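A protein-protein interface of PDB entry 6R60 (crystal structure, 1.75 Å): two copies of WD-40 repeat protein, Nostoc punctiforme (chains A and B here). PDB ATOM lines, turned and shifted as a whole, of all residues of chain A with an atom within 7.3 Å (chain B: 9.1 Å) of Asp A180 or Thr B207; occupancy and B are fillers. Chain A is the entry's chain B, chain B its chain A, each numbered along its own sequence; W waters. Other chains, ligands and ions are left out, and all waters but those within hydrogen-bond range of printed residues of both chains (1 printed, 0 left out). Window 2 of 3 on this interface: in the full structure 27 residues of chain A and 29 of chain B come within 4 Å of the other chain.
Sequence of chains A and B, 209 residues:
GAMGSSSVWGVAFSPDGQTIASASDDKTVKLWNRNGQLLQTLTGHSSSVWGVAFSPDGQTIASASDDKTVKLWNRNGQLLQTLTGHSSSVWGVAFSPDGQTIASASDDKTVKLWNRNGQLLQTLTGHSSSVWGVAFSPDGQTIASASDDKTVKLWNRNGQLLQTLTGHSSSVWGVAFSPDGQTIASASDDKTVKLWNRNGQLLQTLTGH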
ATOM      1  N   LEU A  38      -1.932   4.991   5.388  1.00  0.00           N
ATOM      2  CA  LEU A  38      -1.664   6.000   4.378  1.00  0.00           C
ATOM      3  C   LEU A  38      -0.491   6.885   4.737  1.00  0.00           C
ATOM      4  O   LEU A  38       0.344   7.115   3.888  1.00  0.00           O
ATOM      5  CB  LEU A  38      -2.931   6.821   4.079  1.00  0.00           C
ATOM      6  CG  LEU A  38      -2.755   8.012   3.148  1.00  0.00           C
ATOM      7  CD1 LEU A  38      -2.349   7.539   1.753  1.00  0.00           C
ATOM      8  CD2 LEU A  38      -4.037   8.818   3.099  1.00  0.00           C
ATOM      9  N   SER A 137     -10.371  -0.386   1.256  1.00  0.00           N
ATOM     10  CA  SER A 137     -10.954   0.938   1.132  1.00  0.00           C
ATOM     11  C   SER A 137     -11.768   1.286   2.372  1.00  0.00           C
ATOM     12  O   SER A 137     -12.215   0.399   3.116  1.00  0.00           O
ATOM     13  CB  SER A 137     -11.860   1.040  -0.096  1.00  0.00           C
ATOM     14  OG  SER A 137     -12.996   0.224   0.065  1.00  0.00           O
ATOM     15  N   PRO A 138     -12.020   2.581   2.586  1.00  0.00           N
ATOM     16  CA  PRO A 138     -12.743   2.961   3.791  1.00  0.00           C
ATOM     17  C   PRO A 138     -14.138   2.320   3.928  1.00  0.00           C
ATOM     18  O   PRO A 138     -14.598   2.067   5.048  1.00  0.00           O
ATOM     19  CB  PRO A 138     -12.853   4.484   3.673  1.00  0.00           C
ATOM     20  CG  PRO A 138     -11.678   4.863   2.857  1.00  0.00           C
ATOM     21  CD  PRO A 138     -11.420   3.741   1.902  1.00  0.00           C
ATOM     22  N   ASP A 139     -14.832   2.131   2.807  1.00  0.00           N
ATOM     23  CA  ASP A 139     -16.149   1.516   2.831  1.00  0.00           C
ATOM     24  C   ASP A 139     -16.105  -0.014   2.873  1.00  0.00           C
ATOM     25  O   ASP A 139     -17.141  -0.672   2.935  1.00  0.00           O
ATOM     26  CB  ASP A 139     -17.032   2.037   1.683  1.00  0.00           C
ATOM     27  CG  ASP A 139     -16.693   1.467   0.317  1.00  0.00           C
ATOM     28  OD1 ASP A 139     -15.722   0.684   0.142  1.00  0.00           O
ATOM     29  OD2 ASP A 139     -17.475   1.826  -0.612  1.00  0.00           O
ATOM     30  N   PHE A 177      -5.458   3.671   0.857  1.00  0.00           N
ATOM     31  CA  PHE A 177      -6.474   4.565   0.298  1.00  0.00           C
ATOM     32  C   PHE A 177      -6.475   5.875   1.031  1.00  0.00           C
ATOM     33  O   PHE A 177      -6.272   5.912   2.270  1.00  0.00           O
ATOM     34  CB  PHE A 177      -7.878   3.942   0.435  1.00  0.00           C
ATOM     35  CG  PHE A 177      -8.118   2.761  -0.446  1.00  0.00           C
ATOM     36  CD1 PHE A 177      -7.687   1.503  -0.056  1.00  0.00           C
ATOM     37  CD2 PHE A 177      -8.796   2.899  -1.653  1.00  0.00           C
ATOM     38  CE1 PHE A 177      -7.924   0.399  -0.842  1.00  0.00           C
ATOM     39  CE2 PHE A 177      -9.016   1.790  -2.470  1.00  0.00           C
ATOM     40  CZ  PHE A 177      -8.584   0.558  -2.075  1.00  0.00           C
ATOM     41  N   SER A 178      -6.826   6.932   0.299  1.00  0.00           N
ATOM     42  CA  SER A 178      -7.190   8.178   0.919  1.00  0.00           C
ATOM     43  C   SER A 178      -8.424   7.989   1.836  1.00  0.00           C
ATOM     44  O   SER A 178      -9.185   7.064   1.676  1.00  0.00           O
ATOM     45  CB  SER A 178      -7.458   9.257  -0.114  1.00  0.00           C
ATOM     46  OG  SER A 178      -8.618   8.973  -0.869  1.00  0.00           O
ATOM     47  N   PRO A 179      -8.635   8.906   2.788  1.00  0.00           N
ATOM     48  CA  PRO A 179      -9.752   8.719   3.711  1.00  0.00           C
ATOM     49  C   PRO A 179     -11.130   8.693   3.022  1.00  0.00           C
ATOM     50  O   PRO A 179     -12.043   8.113   3.551  1.00  0.00           O
ATOM     51  CB  PRO A 179      -9.644   9.939   4.643  1.00  0.00           C
ATOM     52  CG  PRO A 179      -8.207  10.324   4.602  1.00  0.00           C
ATOM     53  CD  PRO A 179      -7.708   9.959   3.234  1.00  0.00           C
ATOM     54  N   ASP A 180     -11.289   9.379   1.889  1.00  0.00           N
ATOM     55  CA  ASP A 180     -12.568   9.384   1.156  1.00  0.00           C
ATOM     56  C   ASP A 180     -12.683   8.224   0.193  1.00  0.00           C
ATOM     57  O   ASP A 180     -13.692   8.057  -0.483  1.00  0.00           O
ATOM     58  CB  ASP A 180     -12.815  10.729   0.464  1.00  0.00           C
ATOM     59  CG  ASP A 180     -11.948  10.981  -0.790  1.00  0.00           C
ATOM     60  OD1 ASP A 180     -11.086  10.169  -1.195  1.00  0.00           O
ATOM     61  OD2 ASP A 180     -12.129  12.063  -1.347  1.00  0.00           O
ATOM     62  N   GLY A 181     -11.610   7.478   0.095  1.00  0.00           N
ATOM     63  CA  GLY A 181     -11.574   6.238  -0.683  1.00  0.00           C
ATOM     64  C   GLY A 181     -11.424   6.392  -2.190  1.00  0.00           C
ATOM     65  O   GLY A 181     -11.371   5.389  -2.911  1.00  0.00           O
ATOM     66  N   GLN A 182     -11.257   7.614  -2.682  1.00  0.00           N
ATOM     67  CA  GLN A 182     -11.207   7.839  -4.129  1.00  0.00           C
ATOM     68  C   GLN A 182      -9.782   7.934  -4.731  1.00  0.00           C
ATOM     69  O   GLN A 182      -9.646   8.049  -5.949  1.00  0.00           O
ATOM     70  CB  GLN A 182     -12.037   9.077  -4.523  1.00  0.00           C
ATOM     71  CG  GLN A 182     -13.509   8.996  -4.103  1.00  0.00           C
ATOM     72  CD  GLN A 182     -14.113   7.621  -4.346  1.00  0.00           C
ATOM     73  OE1 GLN A 182     -14.296   7.183  -5.502  1.00  0.00           O
ATOM     74  NE2 GLN A 182     -14.470   6.940  -3.260  1.00  0.00           N
ATOM     75  N   THR A 183      -8.746   7.938  -3.884  1.00  0.00           N
ATOM     76  CA  THR A 183      -7.376   8.012  -4.325  1.00  0.00           C
ATOM     77  C   THR A 183      -6.637   6.866  -3.681  1.00  0.00           C
ATOM     78  O   THR A 183      -6.813   6.559  -2.492  1.00  0.00           O
ATOM     79  CB  THR A 183      -6.692   9.351  -3.953  1.00  0.00           C
ATOM     80  OG1 THR A 183      -7.445  10.439  -4.478  1.00  0.00           O
ATOM     81  CG2 THR A 183      -5.250   9.424  -4.519  1.00  0.00           C
ATOM     82  N   ARG A 198      -9.372   5.502  -9.215  1.00  0.00           N
ATOM     83  CA  ARG A 198      -9.888   4.138  -9.366  1.00  0.00           C
ATOM     84  C   ARG A 198      -9.943   3.640 -10.815  1.00  0.00           C
ATOM     85  O   ARG A 198     -10.041   2.437 -11.025  1.00  0.00           O
ATOM     86  CB  ARG A 198     -11.273   4.028  -8.685  1.00  0.00           C
ATOM     87  CG  ARG A 198     -11.176   3.993  -7.164  1.00  0.00           C
ATOM     88  CD  ARG A 198     -12.506   4.249  -6.494  1.00  0.00           C
ATOM     89  NE  ARG A 198     -12.504   3.940  -5.052  1.00  0.00           N
ATOM     90  CZ  ARG A 198     -12.827   2.761  -4.491  1.00  0.00           C
ATOM     91  NH1 ARG A 198     -13.151   1.715  -5.236  1.00  0.00           N
ATOM     92  NH2 ARG A 198     -12.836   2.639  -3.160  1.00  0.00           N
ATOM     93  N   HIS B 168      -6.303  22.229   8.857  1.00  0.00           N
ATOM     94  CA  HIS B 168      -7.229  21.140   9.227  1.00  0.00           C
ATOM     95  C   HIS B 168      -8.453  21.726   9.998  1.00  0.00           C
ATOM     96  O   HIS B 168      -8.328  22.697  10.727  1.00  0.00           O
ATOM     97  CB  HIS B 168      -6.540  20.062  10.040  1.00  0.00           C
ATOM     98  CG  HIS B 168      -5.674  19.139   9.232  1.00  0.00           C
ATOM     99  ND1 HIS B 168      -6.179  18.302   8.269  1.00  0.00           N
ATOM    100  CD2 HIS B 168      -4.346  18.888   9.289  1.00  0.00           C
ATOM    101  CE1 HIS B 168      -5.206  17.561   7.762  1.00  0.00           C
ATOM    102  NE2 HIS B 168      -4.080  17.913   8.353  1.00  0.00           N
ATOM    103  N   SER B 188      -5.828  14.002   9.910  1.00  0.00           N
ATOM    104  CA  SER B 188      -6.782  14.606  10.805  1.00  0.00           C
ATOM    105  C   SER B 188      -8.127  13.873  10.808  1.00  0.00           C
ATOM    106  O   SER B 188      -8.524  13.231   9.781  1.00  0.00           O
ATOM    107  CB  SER B 188      -6.959  16.063  10.360  1.00  0.00           C
ATOM    108  OG  SER B 188      -8.057  16.697  10.966  1.00  0.00           O
ATOM    109  N   ASP B 190     -10.719  15.338  10.298  1.00  0.00           N
ATOM    110  CA  ASP B 190     -11.475  15.968   9.189  1.00  0.00           C
ATOM    111  C   ASP B 190     -11.450  15.140   7.897  1.00  0.00           C
ATOM    112  O   ASP B 190     -12.069  15.523   6.916  1.00  0.00           O
ATOM    113  CB  ASP B 190     -11.015  17.412   8.914  1.00  0.00           C
ATOM    114  CG  ASP B 190      -9.607  17.503   8.284  1.00  0.00           C
ATOM    115  OD1 ASP B 190      -9.006  16.477   7.840  1.00  0.00           O
ATOM    116  OD2 ASP B 190      -9.102  18.643   8.217  1.00  0.00           O
ATOM    117  N   LYS B 191     -10.812  13.976   7.953  1.00  0.00           N
ATOM    118  CA  LYS B 191     -10.840  12.988   6.871  1.00  0.00           C
ATOM    119  C   LYS B 191      -9.988  13.430   5.696  1.00  0.00           C
ATOM    120  O   LYS B 191     -10.272  13.111   4.530  1.00  0.00           O
ATOM    121  CB  LYS B 191     -12.269  12.663   6.422  1.00  0.00           C
ATOM    122  CG  LYS B 191     -13.276  12.430   7.558  1.00  0.00           C
ATOM    123  CD  LYS B 191     -14.609  11.888   7.082  1.00  0.00           C
ATOM    124  CE  LYS B 191     -14.492  10.521   6.408  1.00  0.00           C
ATOM    125  NZ  LYS B 191     -13.704   9.447   7.095  1.00  0.00           N
ATOM    126  N   THR B 192      -8.942  14.157   6.003  1.00  0.00           N
ATOM    127  CA  THR B 192      -7.972  14.550   5.009  1.00  0.00           C
ATOM    128  C   THR B 192      -6.561  14.265   5.524  1.00  0.00           C
ATOM    129  O   THR B 192      -6.303  14.120   6.736  1.00  0.00           O
ATOM    130  CB  THR B 192      -8.060  16.063   4.617  1.00  0.00           C
ATOM    131  OG1 THR B 192      -7.576  16.880   5.683  1.00  0.00           O
ATOM    132  CG2 THR B 192      -9.498  16.494   4.265  1.00  0.00           C
ATOM    133  N   VAL B 193      -5.653  14.157   4.560  1.00  0.00           N
ATOM    134  CA  VAL B 193      -4.250  14.234   4.813  1.00  0.00           C
ATOM    135  C   VAL B 193      -3.768  15.484   4.085  1.00  0.00           C
ATOM    136  O   VAL B 193      -4.153  15.750   2.935  1.00  0.00           O
ATOM    137  CB  VAL B 193      -3.530  12.968   4.313  1.00  0.00           C
ATOM    138  CG1 VAL B 193      -2.040  13.145   4.336  1.00  0.00           C
ATOM    139  CG2 VAL B 193      -3.944  11.767   5.141  1.00  0.00           C
ATOM    140  N   LYS B 194      -2.935  16.253   4.764  1.00  0.00           N
ATOM    141  CA  LYS B 194      -2.325  17.428   4.144  1.00  0.00           C
ATOM    142  C   LYS B 194      -0.841  17.254   4.075  1.00  0.00           C
ATOM    143  O   LYS B 194      -0.209  16.700   4.992  1.00  0.00           O
ATOM    144  CB  LYS B 194      -2.770  18.695   4.886  1.00  0.00           C
ATOM    145  CG  LYS B 194      -4.212  19.041   4.575  1.00  0.00           C
ATOM    146  CD  LYS B 194      -4.709  20.171   5.473  1.00  0.00           C
ATOM    147  CE  LYS B 194      -6.192  20.370   5.280  1.00  0.00           C
ATOM    148  NZ  LYS B 194      -6.457  21.104   4.013  1.00  0.00           N
ATOM    149  N   GLN B 204      -0.730  20.434  -0.635  1.00  0.00           N
ATOM    150  CA  GLN B 204      -1.875  19.747  -1.210  1.00  0.00           C
ATOM    151  C   GLN B 204      -2.681  19.127  -0.061  1.00  0.00           C
ATOM    152  O   GLN B 204      -2.189  18.829   1.030  1.00  0.00           O
ATOM    153  CB  GLN B 204      -1.446  18.673  -2.265  1.00  0.00           C
ATOM    154  CG  GLN B 204      -0.775  17.435  -1.689  1.00  0.00           C
ATOM    155  CD  GLN B 204      -0.203  16.535  -2.742  1.00  0.00           C
ATOM    156  OE1 GLN B 204       0.894  16.797  -3.174  1.00  0.00           O
ATOM    157  NE2 GLN B 204      -0.939  15.518  -3.196  1.00  0.00           N
ATOM    158  N   THR B 205      -3.930  18.870  -0.393  1.00  0.00           N
ATOM    159  CA  THR B 205      -4.851  18.158   0.464  1.00  0.00           C
ATOM    160  C   THR B 205      -5.270  16.887  -0.237  1.00  0.00           C
ATOM    161  O   THR B 205      -5.677  16.926  -1.401  1.00  0.00           O
ATOM    162  CB  THR B 205      -6.079  19.025   0.727  1.00  0.00           C
ATOM    163  OG1 THR B 205      -5.630  20.211   1.346  1.00  0.00           O
ATOM    164  CG2 THR B 205      -7.081  18.320   1.639  1.00  0.00           C
ATOM    165  N   LEU B 206      -5.192  15.756   0.489  1.00  0.00           N
ATOM    166  CA  LEU B 206      -5.695  14.496   0.006  1.00  0.00           C
ATOM    167  C   LEU B 206      -7.005  14.184   0.723  1.00  0.00           C
ATOM    168  O   LEU B 206      -7.008  14.026   1.949  1.00  0.00           O
ATOM    169  CB  LEU B 206      -4.625  13.406   0.281  1.00  0.00           C
ATOM    170  CG  LEU B 206      -4.669  12.184  -0.660  1.00  0.00           C
ATOM    171  CD1 LEU B 206      -4.041  12.553  -1.985  1.00  0.00           C
ATOM    172  CD2 LEU B 206      -3.963  10.956  -0.126  1.00  0.00           C
ATOM    173  N   THR B 207      -8.124  14.124  -0.023  1.00  0.00           N
ATOM    174  CA  THR B 207      -9.418  13.769   0.575  1.00  0.00           C
ATOM    175  C   THR B 207      -9.590  12.263   0.420  1.00  0.00           C
ATOM    176  O   THR B 207     -10.196  11.633   1.282  1.00  0.00           O
ATOM    177  CB  THR B 207     -10.652  14.508  -0.031  1.00  0.00           C
ATOM    178  OG1 THR B 207     -10.748  14.238  -1.443  1.00  0.00           O
ATOM    179  CG2 THR B 207     -10.567  16.004   0.217  1.00  0.00           C
HETATM  180  O   HOH W   1     -11.630   7.192   6.035  1.00  0.00           O
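Of the 12 printed residues of chain A, 4 touch a printed residue of chain B. Among the printed residues, 7 pairs touch across the chains.
Asp A180 touches one residue of chain B. Thr B207 touches just these residues of chain A: Ser A178 (3.7 Å), Pro A179 (3.5 Å) and Asp A180 (2.6 Å). Of chain B, only Lys B191 and Thr B207 come within 4 Å of Pro A179. Of the printed residues of chain A, Lys B191 touches Pro A179 (3.2 Å). Printed residues of chain A within 4 Å of Val B193: Leu A38 (3.6 Å). Printed residues of chain B within 4 Å of Leu A38: Val B193 (3.6 Å) and Leu B206 (3.9 Å). Of the printed residues of chain B, Ser A178 touches Leu B206 and Thr B207. Thr A183 touches none of the printed residues of chain B. His B168 touches none of the printed residues of chain A.
O of Thr B207 is in hydrogen-bond range of N of Asp A180, at 2.6 Å. The backbone nitrogen (N) of Pro A179 lies close to the backbone carbonyl oxygen (O) of Thr B207.
No position is printed for both chains. Of the 7 pairs that touch across the chains among the printed residues, none has its exchanged pair printed and touching as well.
The backbone carbonyl oxygen of Val B193 sits at hydrogen-bond distance from the backbone NH of Leu B206 (2.7 Å). The side-chain hydroxyl (OG) of Ser A178 lies within hydrogen-bond range of the side-chain carboxylate (OD1) of Asp A180, at 2.8 Å. N of Gly A181 lies within hydrogen-bond range of OG of Ser A178 (3.5 Å). OG of Ser A178 sits at hydrogen-bond distance from N of Gln A182 (3.5 Å). The backbone NH of Ser A178 is in hydrogen-bond range of the backbone carbonyl oxygen of Thr A183. The side-chain carboxylate (OD1) of Asp A180 sits at hydrogen-bond distance from the backbone NH (N) of Gln A182, 3.0 Å away.
CD2 of Leu A38 touches CG2 of Val B193, at 3.6 Å. CD2 of Leu A38 touches CD2 of Leu B206 (3.9 Å). Leu B206 touches Ser A178. Ser A178 touches Thr B207. Pro A179 touches Lys B191.
Water W1 bridges O of Pro A179 (2.7 Å) and NZ of Lys B191 (3.2 Å).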
